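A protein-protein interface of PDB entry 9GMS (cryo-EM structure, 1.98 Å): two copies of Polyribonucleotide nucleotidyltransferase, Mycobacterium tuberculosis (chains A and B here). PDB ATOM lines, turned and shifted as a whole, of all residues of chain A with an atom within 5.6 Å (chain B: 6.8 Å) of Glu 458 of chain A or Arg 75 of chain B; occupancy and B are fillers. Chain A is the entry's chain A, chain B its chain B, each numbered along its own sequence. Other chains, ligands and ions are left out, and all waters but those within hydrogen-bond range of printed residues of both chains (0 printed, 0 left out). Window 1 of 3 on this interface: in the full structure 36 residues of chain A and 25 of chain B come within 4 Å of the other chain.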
ATOM      1  N   GLN A 377     -33.275   5.666  28.346  1.00  0.00           N
ATOM      2  CA  GLN A 377     -32.343   5.669  29.471  1.00  0.00           C
ATOM      3  C   GLN A 377     -31.083   6.417  29.070  1.00  0.00           C
ATOM      4  O   GLN A 377     -30.410   6.012  28.112  1.00  0.00           O
ATOM      5  CB  GLN A 377     -31.996   4.240  29.895  1.00  0.00           C
ATOM      6  CG  GLN A 377     -31.048   4.146  31.074  1.00  0.00           C
ATOM      7  CD  GLN A 377     -30.732   2.713  31.453  1.00  0.00           C
ATOM      8  OE1 GLN A 377     -30.007   2.020  30.749  1.00  0.00           O
ATOM      9  NE2 GLN A 377     -31.279   2.264  32.570  1.00  0.00           N
ATOM     10  N   ILE A 378     -30.755   7.472  29.826  1.00  0.00           N
ATOM     11  CA  ILE A 378     -29.633   8.361  29.545  1.00  0.00           C
ATOM     12  C   ILE A 378     -28.703   8.407  30.753  1.00  0.00           C
ATOM     13  O   ILE A 378     -29.158   8.521  31.896  1.00  0.00           O
ATOM     14  CB  ILE A 378     -30.108   9.789  29.191  1.00  0.00           C
ATOM     15  CG1 ILE A 378     -31.154   9.776  28.068  1.00  0.00           C
ATOM     16  CG2 ILE A 378     -28.929  10.660  28.808  1.00  0.00           C
ATOM     17  CD1 ILE A 378     -30.707   9.116  26.782  1.00  0.00           C
ATOM     18  N   LEU A 379     -27.398   8.333  30.487  1.00  0.00           N
ATOM     19  CA  LEU A 379     -26.349   8.477  31.494  1.00  0.00           C
ATOM     20  C   LEU A 379     -25.553   9.743  31.197  1.00  0.00           C
ATOM     21  O   LEU A 379     -25.008   9.888  30.100  1.00  0.00           O
ATOM     22  CB  LEU A 379     -25.425   7.257  31.497  1.00  0.00           C
ATOM     23  CG  LEU A 379     -24.155   7.331  32.356  1.00  0.00           C
ATOM     24  CD1 LEU A 379     -24.497   7.358  33.830  1.00  0.00           C
ATOM     25  CD2 LEU A 379     -23.211   6.183  32.052  1.00  0.00           C
ATOM     26  N   GLY A 380     -25.473  10.642  32.169  1.00  0.00           N
ATOM     27  CA  GLY A 380     -24.765  11.907  32.003  1.00  0.00           C
ATOM     28  C   GLY A 380     -23.609  12.037  32.973  1.00  0.00           C
ATOM     29  O   GLY A 380     -23.734  11.678  34.144  1.00  0.00           O
ATOM     30  N   HIS A 407     -21.364  16.816  24.388  1.00  0.00           N
ATOM     31  CA  HIS A 407     -21.202  15.768  23.389  1.00  0.00           C
ATOM     32  C   HIS A 407     -22.209  14.653  23.634  1.00  0.00           C
ATOM     33  O   HIS A 407     -22.431  14.248  24.777  1.00  0.00           O
ATOM     34  CB  HIS A 407     -19.781  15.199  23.418  1.00  0.00           C
ATOM     35  CG  HIS A 407     -18.722  16.200  23.072  1.00  0.00           C
ATOM     36  ND1 HIS A 407     -17.471  16.184  23.647  1.00  0.00           N
ATOM     37  CD2 HIS A 407     -18.723  17.240  22.206  1.00  0.00           C
ATOM     38  CE1 HIS A 407     -16.749  17.172  23.155  1.00  0.00           C
ATOM     39  NE2 HIS A 407     -17.485  17.830  22.280  1.00  0.00           N
ATOM     40  N   ASN A 409     -23.739  10.741  22.402  1.00  0.00           N
ATOM     41  CA  ASN A 409     -23.355   9.464  21.801  1.00  0.00           C
ATOM     42  C   ASN A 409     -24.548   8.518  21.714  1.00  0.00           C
ATOM     43  O   ASN A 409     -25.331   8.393  22.663  1.00  0.00           O
ATOM     44  CB  ASN A 409     -22.236   8.781  22.600  1.00  0.00           C
ATOM     45  CG  ASN A 409     -20.938   9.554  22.569  1.00  0.00           C
ATOM     46  OD1 ASN A 409     -20.316   9.701  21.523  1.00  0.00           O
ATOM     47  ND2 ASN A 409     -20.513  10.039  23.725  1.00  0.00           N
ATOM     48  N   PRO A 411     -24.906   4.671  20.634  1.00  0.00           N
ATOM     49  CA  PRO A 411     -24.276   3.412  20.199  1.00  0.00           C
ATOM     50  C   PRO A 411     -25.278   2.461  19.566  1.00  0.00           C
ATOM     51  O   PRO A 411     -26.484   2.542  19.838  1.00  0.00           O
ATOM     52  CB  PRO A 411     -23.710   2.837  21.504  1.00  0.00           C
ATOM     53  CG  PRO A 411     -24.600   3.368  22.550  1.00  0.00           C
ATOM     54  CD  PRO A 411     -25.009   4.743  22.101  1.00  0.00           C
ATOM     55  N   VAL A 456     -21.100  14.992  28.838  1.00  0.00           N
ATOM     56  CA  VAL A 456     -21.250  13.882  27.904  1.00  0.00           C
ATOM     57  C   VAL A 456     -22.552  13.155  28.212  1.00  0.00           C
ATOM     58  O   VAL A 456     -22.824  12.827  29.371  1.00  0.00           O
ATOM     59  CB  VAL A 456     -20.059  12.905  27.975  1.00  0.00           C
ATOM     60  CG1 VAL A 456     -20.263  11.753  27.010  1.00  0.00           C
ATOM     61  CG2 VAL A 456     -18.759  13.620  27.675  1.00  0.00           C
ATOM     62  N   SER A 457     -23.352  12.910  27.177  1.00  0.00           N
ATOM     63  CA  SER A 457     -24.575  12.123  27.269  1.00  0.00           C
ATOM     64  C   SER A 457     -24.410  10.855  26.447  1.00  0.00           C
ATOM     65  O   SER A 457     -23.943  10.909  25.306  1.00  0.00           O
ATOM     66  CB  SER A 457     -25.788  12.903  26.758  1.00  0.00           C
ATOM     67  OG  SER A 457     -26.040  14.045  27.548  1.00  0.00           O
ATOM     68  N   GLU A 458     -24.779   9.721  27.028  1.00  0.00           N
ATOM     69  CA  GLU A 458     -24.729   8.432  26.351  1.00  0.00           C
ATOM     70  C   GLU A 458     -26.116   7.812  26.363  1.00  0.00           C
ATOM     71  O   GLU A 458     -26.697   7.609  27.432  1.00  0.00           O
ATOM     72  CB  GLU A 458     -23.708   7.516  27.017  1.00  0.00           C
ATOM     73  CG  GLU A 458     -22.305   8.084  26.955  1.00  0.00           C
ATOM     74  CD  GLU A 458     -21.292   7.217  27.633  1.00  0.00           C
ATOM     75  OE1 GLU A 458     -21.700   6.292  28.366  1.00  0.00           O
ATOM     76  OE2 GLU A 458     -20.085   7.459  27.432  1.00  0.00           O
ATOM     77  N   ALA A 459     -26.643   7.496  25.180  1.00  0.00           N
ATOM     78  CA  ALA A 459     -27.984   6.923  25.070  1.00  0.00           C
ATOM     79  C   ALA A 459     -27.899   5.419  25.284  1.00  0.00           C
ATOM     80  O   ALA A 459     -27.771   4.643  24.339  1.00  0.00           O
ATOM     81  CB  ALA A 459     -28.599   7.255  23.719  1.00  0.00           C
ATOM     82  N   LEU A 460     -27.973   4.992  26.547  1.00  0.00           N
ATOM     83  CA  LEU A 460     -27.924   3.562  26.829  1.00  0.00           C
ATOM     84  C   LEU A 460     -29.184   2.852  26.358  1.00  0.00           C
ATOM     85  O   LEU A 460     -29.124   1.669  26.012  1.00  0.00           O
ATOM     86  CB  LEU A 460     -27.713   3.315  28.321  1.00  0.00           C
ATOM     87  CG  LEU A 460     -26.431   3.894  28.923  1.00  0.00           C
ATOM     88  CD1 LEU A 460     -26.311   3.501  30.377  1.00  0.00           C
ATOM     89  CD2 LEU A 460     -25.203   3.454  28.148  1.00  0.00           C
ATOM     90  N   GLY A 461     -30.325   3.540  26.328  1.00  0.00           N
ATOM     91  CA  GLY A 461     -31.514   2.935  25.749  1.00  0.00           C
ATOM     92  C   GLY A 461     -32.396   3.945  25.047  1.00  0.00           C
ATOM     93  O   GLY A 461     -32.676   4.999  25.617  1.00  0.00           O
ATOM     94  N   LEU B  50     -18.578  -1.215  31.568  1.00  0.00           N
ATOM     95  CA  LEU B  50     -19.806  -1.815  31.053  1.00  0.00           C
ATOM     96  C   LEU B  50     -19.524  -2.569  29.762  1.00  0.00           C
ATOM     97  O   LEU B  50     -18.784  -2.081  28.905  1.00  0.00           O
ATOM     98  CB  LEU B  50     -20.885  -0.745  30.789  1.00  0.00           C
ATOM     99  CG  LEU B  50     -22.125  -1.156  29.976  1.00  0.00           C
ATOM    100  CD1 LEU B  50     -23.065  -2.030  30.788  1.00  0.00           C
ATOM    101  CD2 LEU B  50     -22.857   0.060  29.446  1.00  0.00           C
ATOM    102  N   GLU B  73     -14.050   1.410  24.042  1.00  0.00           N
ATOM    103  CA  GLU B  73     -14.271   2.851  24.073  1.00  0.00           C
ATOM    104  C   GLU B  73     -13.722   3.396  25.386  1.00  0.00           C
ATOM    105  O   GLU B  73     -14.322   3.191  26.448  1.00  0.00           O
ATOM    106  CB  GLU B  73     -15.757   3.177  23.935  1.00  0.00           C
ATOM    107  CG  GLU B  73     -16.415   2.633  22.682  1.00  0.00           C
ATOM    108  CD  GLU B  73     -16.291   3.578  21.506  1.00  0.00           C
ATOM    109  OE1 GLU B  73     -17.139   4.485  21.377  1.00  0.00           O
ATOM    110  OE2 GLU B  73     -15.340   3.421  20.713  1.00  0.00           O
ATOM    111  N   GLU B  74     -12.594   4.099  25.311  1.00  0.00           N
ATOM    112  CA  GLU B  74     -11.977   4.734  26.475  1.00  0.00           C
ATOM    113  C   GLU B  74     -12.502   6.163  26.581  1.00  0.00           C
ATOM    114  O   GLU B  74     -12.240   6.991  25.708  1.00  0.00           O
ATOM    115  CB  GLU B  74     -10.455   4.730  26.359  1.00  0.00           C
ATOM    116  CG  GLU B  74      -9.806   3.364  26.218  1.00  0.00           C
ATOM    117  CD  GLU B  74      -8.294   3.453  26.104  1.00  0.00           C
ATOM    118  OE1 GLU B  74      -7.785   4.531  25.751  1.00  0.00           O
ATOM    119  OE2 GLU B  74      -7.607   2.447  26.372  1.00  0.00           O
ATOM    120  N   ARG B  75     -13.231   6.457  27.652  1.00  0.00           N
ATOM    121  CA  ARG B  75     -13.779   7.786  27.887  1.00  0.00           C
ATOM    122  C   ARG B  75     -12.835   8.576  28.782  1.00  0.00           C
ATOM    123  O   ARG B  75     -12.417   8.085  29.834  1.00  0.00           O
ATOM    124  CB  ARG B  75     -15.163   7.704  28.531  1.00  0.00           C
ATOM    125  CG  ARG B  75     -16.244   7.160  27.624  1.00  0.00           C
ATOM    126  CD  ARG B  75     -16.562   8.126  26.499  1.00  0.00           C
ATOM    127  NE  ARG B  75     -17.727   7.705  25.729  1.00  0.00           N
ATOM    128  CZ  ARG B  75     -17.679   7.063  24.569  1.00  0.00           C
ATOM    129  NH1 ARG B  75     -16.530   6.754  23.992  1.00  0.00           N
ATOM    130  NH2 ARG B  75     -18.816   6.721  23.972  1.00  0.00           N
ATOM    131  N   MET B  76     -12.510   9.802  28.369  1.00  0.00           N
ATOM    132  CA  MET B  76     -11.535  10.589  29.109  1.00  0.00           C
ATOM    133  C   MET B  76     -12.046  11.013  30.480  1.00  0.00           C
ATOM    134  O   MET B  76     -11.237  11.194  31.396  1.00  0.00           O
ATOM    135  CB  MET B  76     -11.138  11.822  28.299  1.00  0.00           C
ATOM    136  CG  MET B  76      -9.711  12.267  28.519  1.00  0.00           C
ATOM    137  SD  MET B  76      -8.493  11.042  27.998  1.00  0.00           S
ATOM    138  CE  MET B  76      -7.668  10.767  29.552  1.00  0.00           C
ATOM    139  N   TYR B  77     -13.361  11.147  30.660  1.00  0.00           N
ATOM    140  CA  TYR B  77     -13.868  11.508  31.977  1.00  0.00           C
ATOM    141  C   TYR B  77     -13.637  10.408  33.004  1.00  0.00           C
ATOM    142  O   TYR B  77     -13.813  10.655  34.198  1.00  0.00           O
ATOM    143  CB  TYR B  77     -15.357  11.872  31.921  1.00  0.00           C
ATOM    144  CG  TYR B  77     -16.287  10.829  31.338  1.00  0.00           C
ATOM    145  CD1 TYR B  77     -16.570   9.654  32.019  1.00  0.00           C
ATOM    146  CD2 TYR B  77     -16.914  11.043  30.122  1.00  0.00           C
ATOM    147  CE1 TYR B  77     -17.427   8.714  31.492  1.00  0.00           C
ATOM    148  CE2 TYR B  77     -17.774  10.111  29.588  1.00  0.00           C
ATOM    149  CZ  TYR B  77     -18.029   8.949  30.277  1.00  0.00           C
ATOM    150  OH  TYR B  77     -18.882   8.019  29.742  1.00  0.00           O
ATOM    151  N   ALA B  78     -13.250   9.204  32.575  1.00  0.00           N
ATOM    152  CA  ALA B  78     -12.880   8.179  33.540  1.00  0.00           C
ATOM    153  C   ALA B  78     -11.606   8.554  34.289  1.00  0.00           C
ATOM    154  O   ALA B  78     -11.366   8.053  35.391  1.00  0.00           O
ATOM    155  CB  ALA B  78     -12.717   6.826  32.846  1.00  0.00           C
ATOM    156  N   ALA B  79     -10.777   9.424  33.710  1.00  0.00           N
ATOM    157  CA  ALA B  79      -9.583   9.929  34.374  1.00  0.00           C
ATOM    158  C   ALA B  79      -9.787  11.308  34.991  1.00  0.00           C
ATOM    159  O   ALA B  79      -8.868  11.825  35.629  1.00  0.00           O
ATOM    160  CB  ALA B  79      -8.414   9.986  33.388  1.00  0.00           C
ATOM    161  N   GLY B  80     -10.965  11.898  34.836  1.00  0.00           N
ATOM    162  CA  GLY B  80     -11.239  13.230  35.349  1.00  0.00           C
ATOM    163  C   GLY B  80     -10.511  14.379  34.682  1.00  0.00           C
ATOM    164  O   GLY B  80     -10.027  15.278  35.377  1.00  0.00           O
ATOM    165  N   ARG B  81     -10.427  14.387  33.353  1.00  0.00           N
ATOM    166  CA  ARG B  81      -9.874  15.541  32.654  1.00  0.00           C
ATOM    167  C   ARG B  81     -10.437  15.597  31.240  1.00  0.00           C
ATOM    168  O   ARG B  81     -11.081  14.659  30.768  1.00  0.00           O
ATOM    169  CB  ARG B  81      -8.342  15.511  32.649  1.00  0.00           C
ATOM    170  CG  ARG B  81      -7.713  14.445  31.795  1.00  0.00           C
ATOM    171  CD  ARG B  81      -6.200  14.533  31.885  1.00  0.00           C
ATOM    172  NE  ARG B  81      -5.543  13.620  30.960  1.00  0.00           N
ATOM    173  CZ  ARG B  81      -5.118  12.402  31.270  1.00  0.00           C
ATOM    174  NH1 ARG B  81      -5.229  11.920  32.497  1.00  0.00           N
ATOM    175  NH2 ARG B  81      -4.570  11.648  30.325  1.00  0.00           N
ATOM    176  N   GLU B  90     -12.733  12.603  21.888  1.00  0.00           N
ATOM    177  CA  GLU B  90     -11.990  11.377  21.612  1.00  0.00           C
ATOM    178  C   GLU B  90     -12.071  11.014  20.134  1.00  0.00           C
ATOM    179  O   GLU B  90     -13.142  11.056  19.526  1.00  0.00           O
ATOM    180  CB  GLU B  90     -12.527  10.212  22.450  1.00  0.00           C
ATOM    181  CG  GLU B  90     -12.380  10.366  23.959  1.00  0.00           C
ATOM    182  CD  GLU B  90     -13.567  11.055  24.608  1.00  0.00           C
ATOM    183  OE1 GLU B  90     -14.417  11.603  23.883  1.00  0.00           O
ATOM    184  OE2 GLU B  90     -13.650  11.041  25.851  1.00  0.00           O
ATOM    185  N   THR B 125     -17.134  -0.205  27.313  1.00  0.00           N
ATOM    186  CA  THR B 125     -16.942   1.215  27.586  1.00  0.00           C
ATOM    187  C   THR B 125     -16.341   1.397  28.974  1.00  0.00           C
ATOM    188  O   THR B 125     -16.878   0.873  29.954  1.00  0.00           O
ATOM    189  CB  THR B 125     -18.269   1.973  27.492  1.00  0.00           C
ATOM    190  OG1 THR B 125     -18.902   1.687  26.242  1.00  0.00           O
ATOM    191  CG2 THR B 125     -18.045   3.471  27.608  1.00  0.00           C
ATOM    192  N   ILE B 126     -15.243   2.146  29.060  1.00  0.00           N
ATOM    193  CA  ILE B 126     -14.566   2.381  30.333  1.00  0.00           C
ATOM    194  C   ILE B 126     -15.188   3.603  31.002  1.00  0.00           C
ATOM    195  O   ILE B 126     -15.175   4.702  30.438  1.00  0.00           O
ATOM    196  CB  ILE B 126     -13.054   2.575  30.139  1.00  0.00           C
ATOM    197  CG1 ILE B 126     -12.469   1.506  29.212  1.00  0.00           C
ATOM    198  CG2 ILE B 126     -12.347   2.546  31.479  1.00  0.00           C
ATOM    199  CD1 ILE B 126     -12.732   0.087  29.645  1.00  0.00           C
ATOM    200  N   LEU B 127     -15.716   3.419  32.210  1.00  0.00           N
ATOM    201  CA  LEU B 127     -16.441   4.473  32.914  1.00  0.00           C
ATOM    202  C   LEU B 127     -15.668   5.092  34.069  1.00  0.00           C
ATOM    203  O   LEU B 127     -15.752   6.303  34.268  1.00  0.00           O
ATOM    204  CB  LEU B 127     -17.778   3.935  33.436  1.00  0.00           C
ATOM    205  CG  LEU B 127     -18.722   3.327  32.390  1.00  0.00           C
ATOM    206  CD1 LEU B 127     -19.988   2.809  33.044  1.00  0.00           C
ATOM    207  CD2 LEU B 127     -19.064   4.319  31.296  1.00  0.00           C
ATOM    208  N   SER B 128     -14.917   4.313  34.847  1.00  0.00           N
ATOM    209  CA  SER B 128     -14.177   4.882  35.969  1.00  0.00           C
ATOM    210  C   SER B 128     -12.917   4.067  36.222  1.00  0.00           C
ATOM    211  O   SER B 128     -12.979   2.837  36.261  1.00  0.00           O
ATOM    212  CB  SER B 128     -15.051   4.917  37.227  1.00  0.00           C
ATOM    213  OG  SER B 128     -14.326   5.373  38.349  1.00  0.00           O
ATOM    214  N   LEU B 396      -5.692   7.158  28.993  1.00  0.00           N
ATOM    215  CA  LEU B 396      -6.134   6.768  30.329  1.00  0.00           C
ATOM    216  C   LEU B 396      -5.016   6.116  31.128  1.00  0.00           C
ATOM    217  O   LEU B 396      -4.862   6.393  32.322  1.00  0.00           O
ATOM    218  CB  LEU B 396      -7.318   5.808  30.235  1.00  0.00           C
ATOM    219  CG  LEU B 396      -8.703   6.389  29.980  1.00  0.00           C
ATOM    220  CD1 LEU B 396      -9.718   5.267  29.953  1.00  0.00           C
ATOM    221  CD2 LEU B 396      -9.076   7.420  31.031  1.00  0.00           C
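O of Leu 379 of chain A is in hydrogen-bond range of N of Glu 458 of chain A, at 3.1 Å.
The backbone NH (N) of Asn 409 of chain A is in hydrogen-bond range of the backbone carbonyl oxygen (O) of Ser 457 of chain A, 2.9 Å away.
The backbone NH of Ala 459 of chain A lies within hydrogen-bond range of the backbone carbonyl oxygen of Asn 409 of chain A (3.0 Å).
The side-chain carboxylate (OE1) of Glu 73 of chain B is in salt-bridge range of the guanidinium group (NH1) of Arg 75 of chain B, 3.5 Å away.
The side-chain carboxylate of Glu 458 of chain A is in salt-bridge range of the guanidinium group of Arg 75 of chain B, at 2.9 Å.
The side-chain carboxylate of Glu 458 of chain A is in hydrogen-bond range of the side-chain hydroxyl of Tyr 77 of chain B, at 2.7 Å.
No position is printed for both chains.
Of the 16 printed residues of chain B, 2 touch a printed residue of chain A.
Glu 458 of chain A touches two residues of chain B.
Of chain A, only Asn 409 (3.7 Å) and Glu 458 (2.9 Å) come within 4 Å of Arg 75 of chain B.
Of the printed residues of chain A, Tyr 77 of chain B touches Val 456 (3.9 Å) and Glu 458 (2.7 Å).
Of the printed residues of chain B, Asn 409 of chain A touches Arg 75.
Glu 74 of chain B touches none of the printed residues of chain A.
Ala 459 of chain A touches none of the printed residues of chain B.
The nearest printed residue of chain A that does not touch Tyr 77 of chain B is Leu 379 of chain A (5.2 Å).
Among the printed residues, merely in contact across the chains: Asn 409 of chain A with Arg 75 of chain B (3.7 Å) and Val 456 of chain A with Tyr 77 of chain B (3.9 Å).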
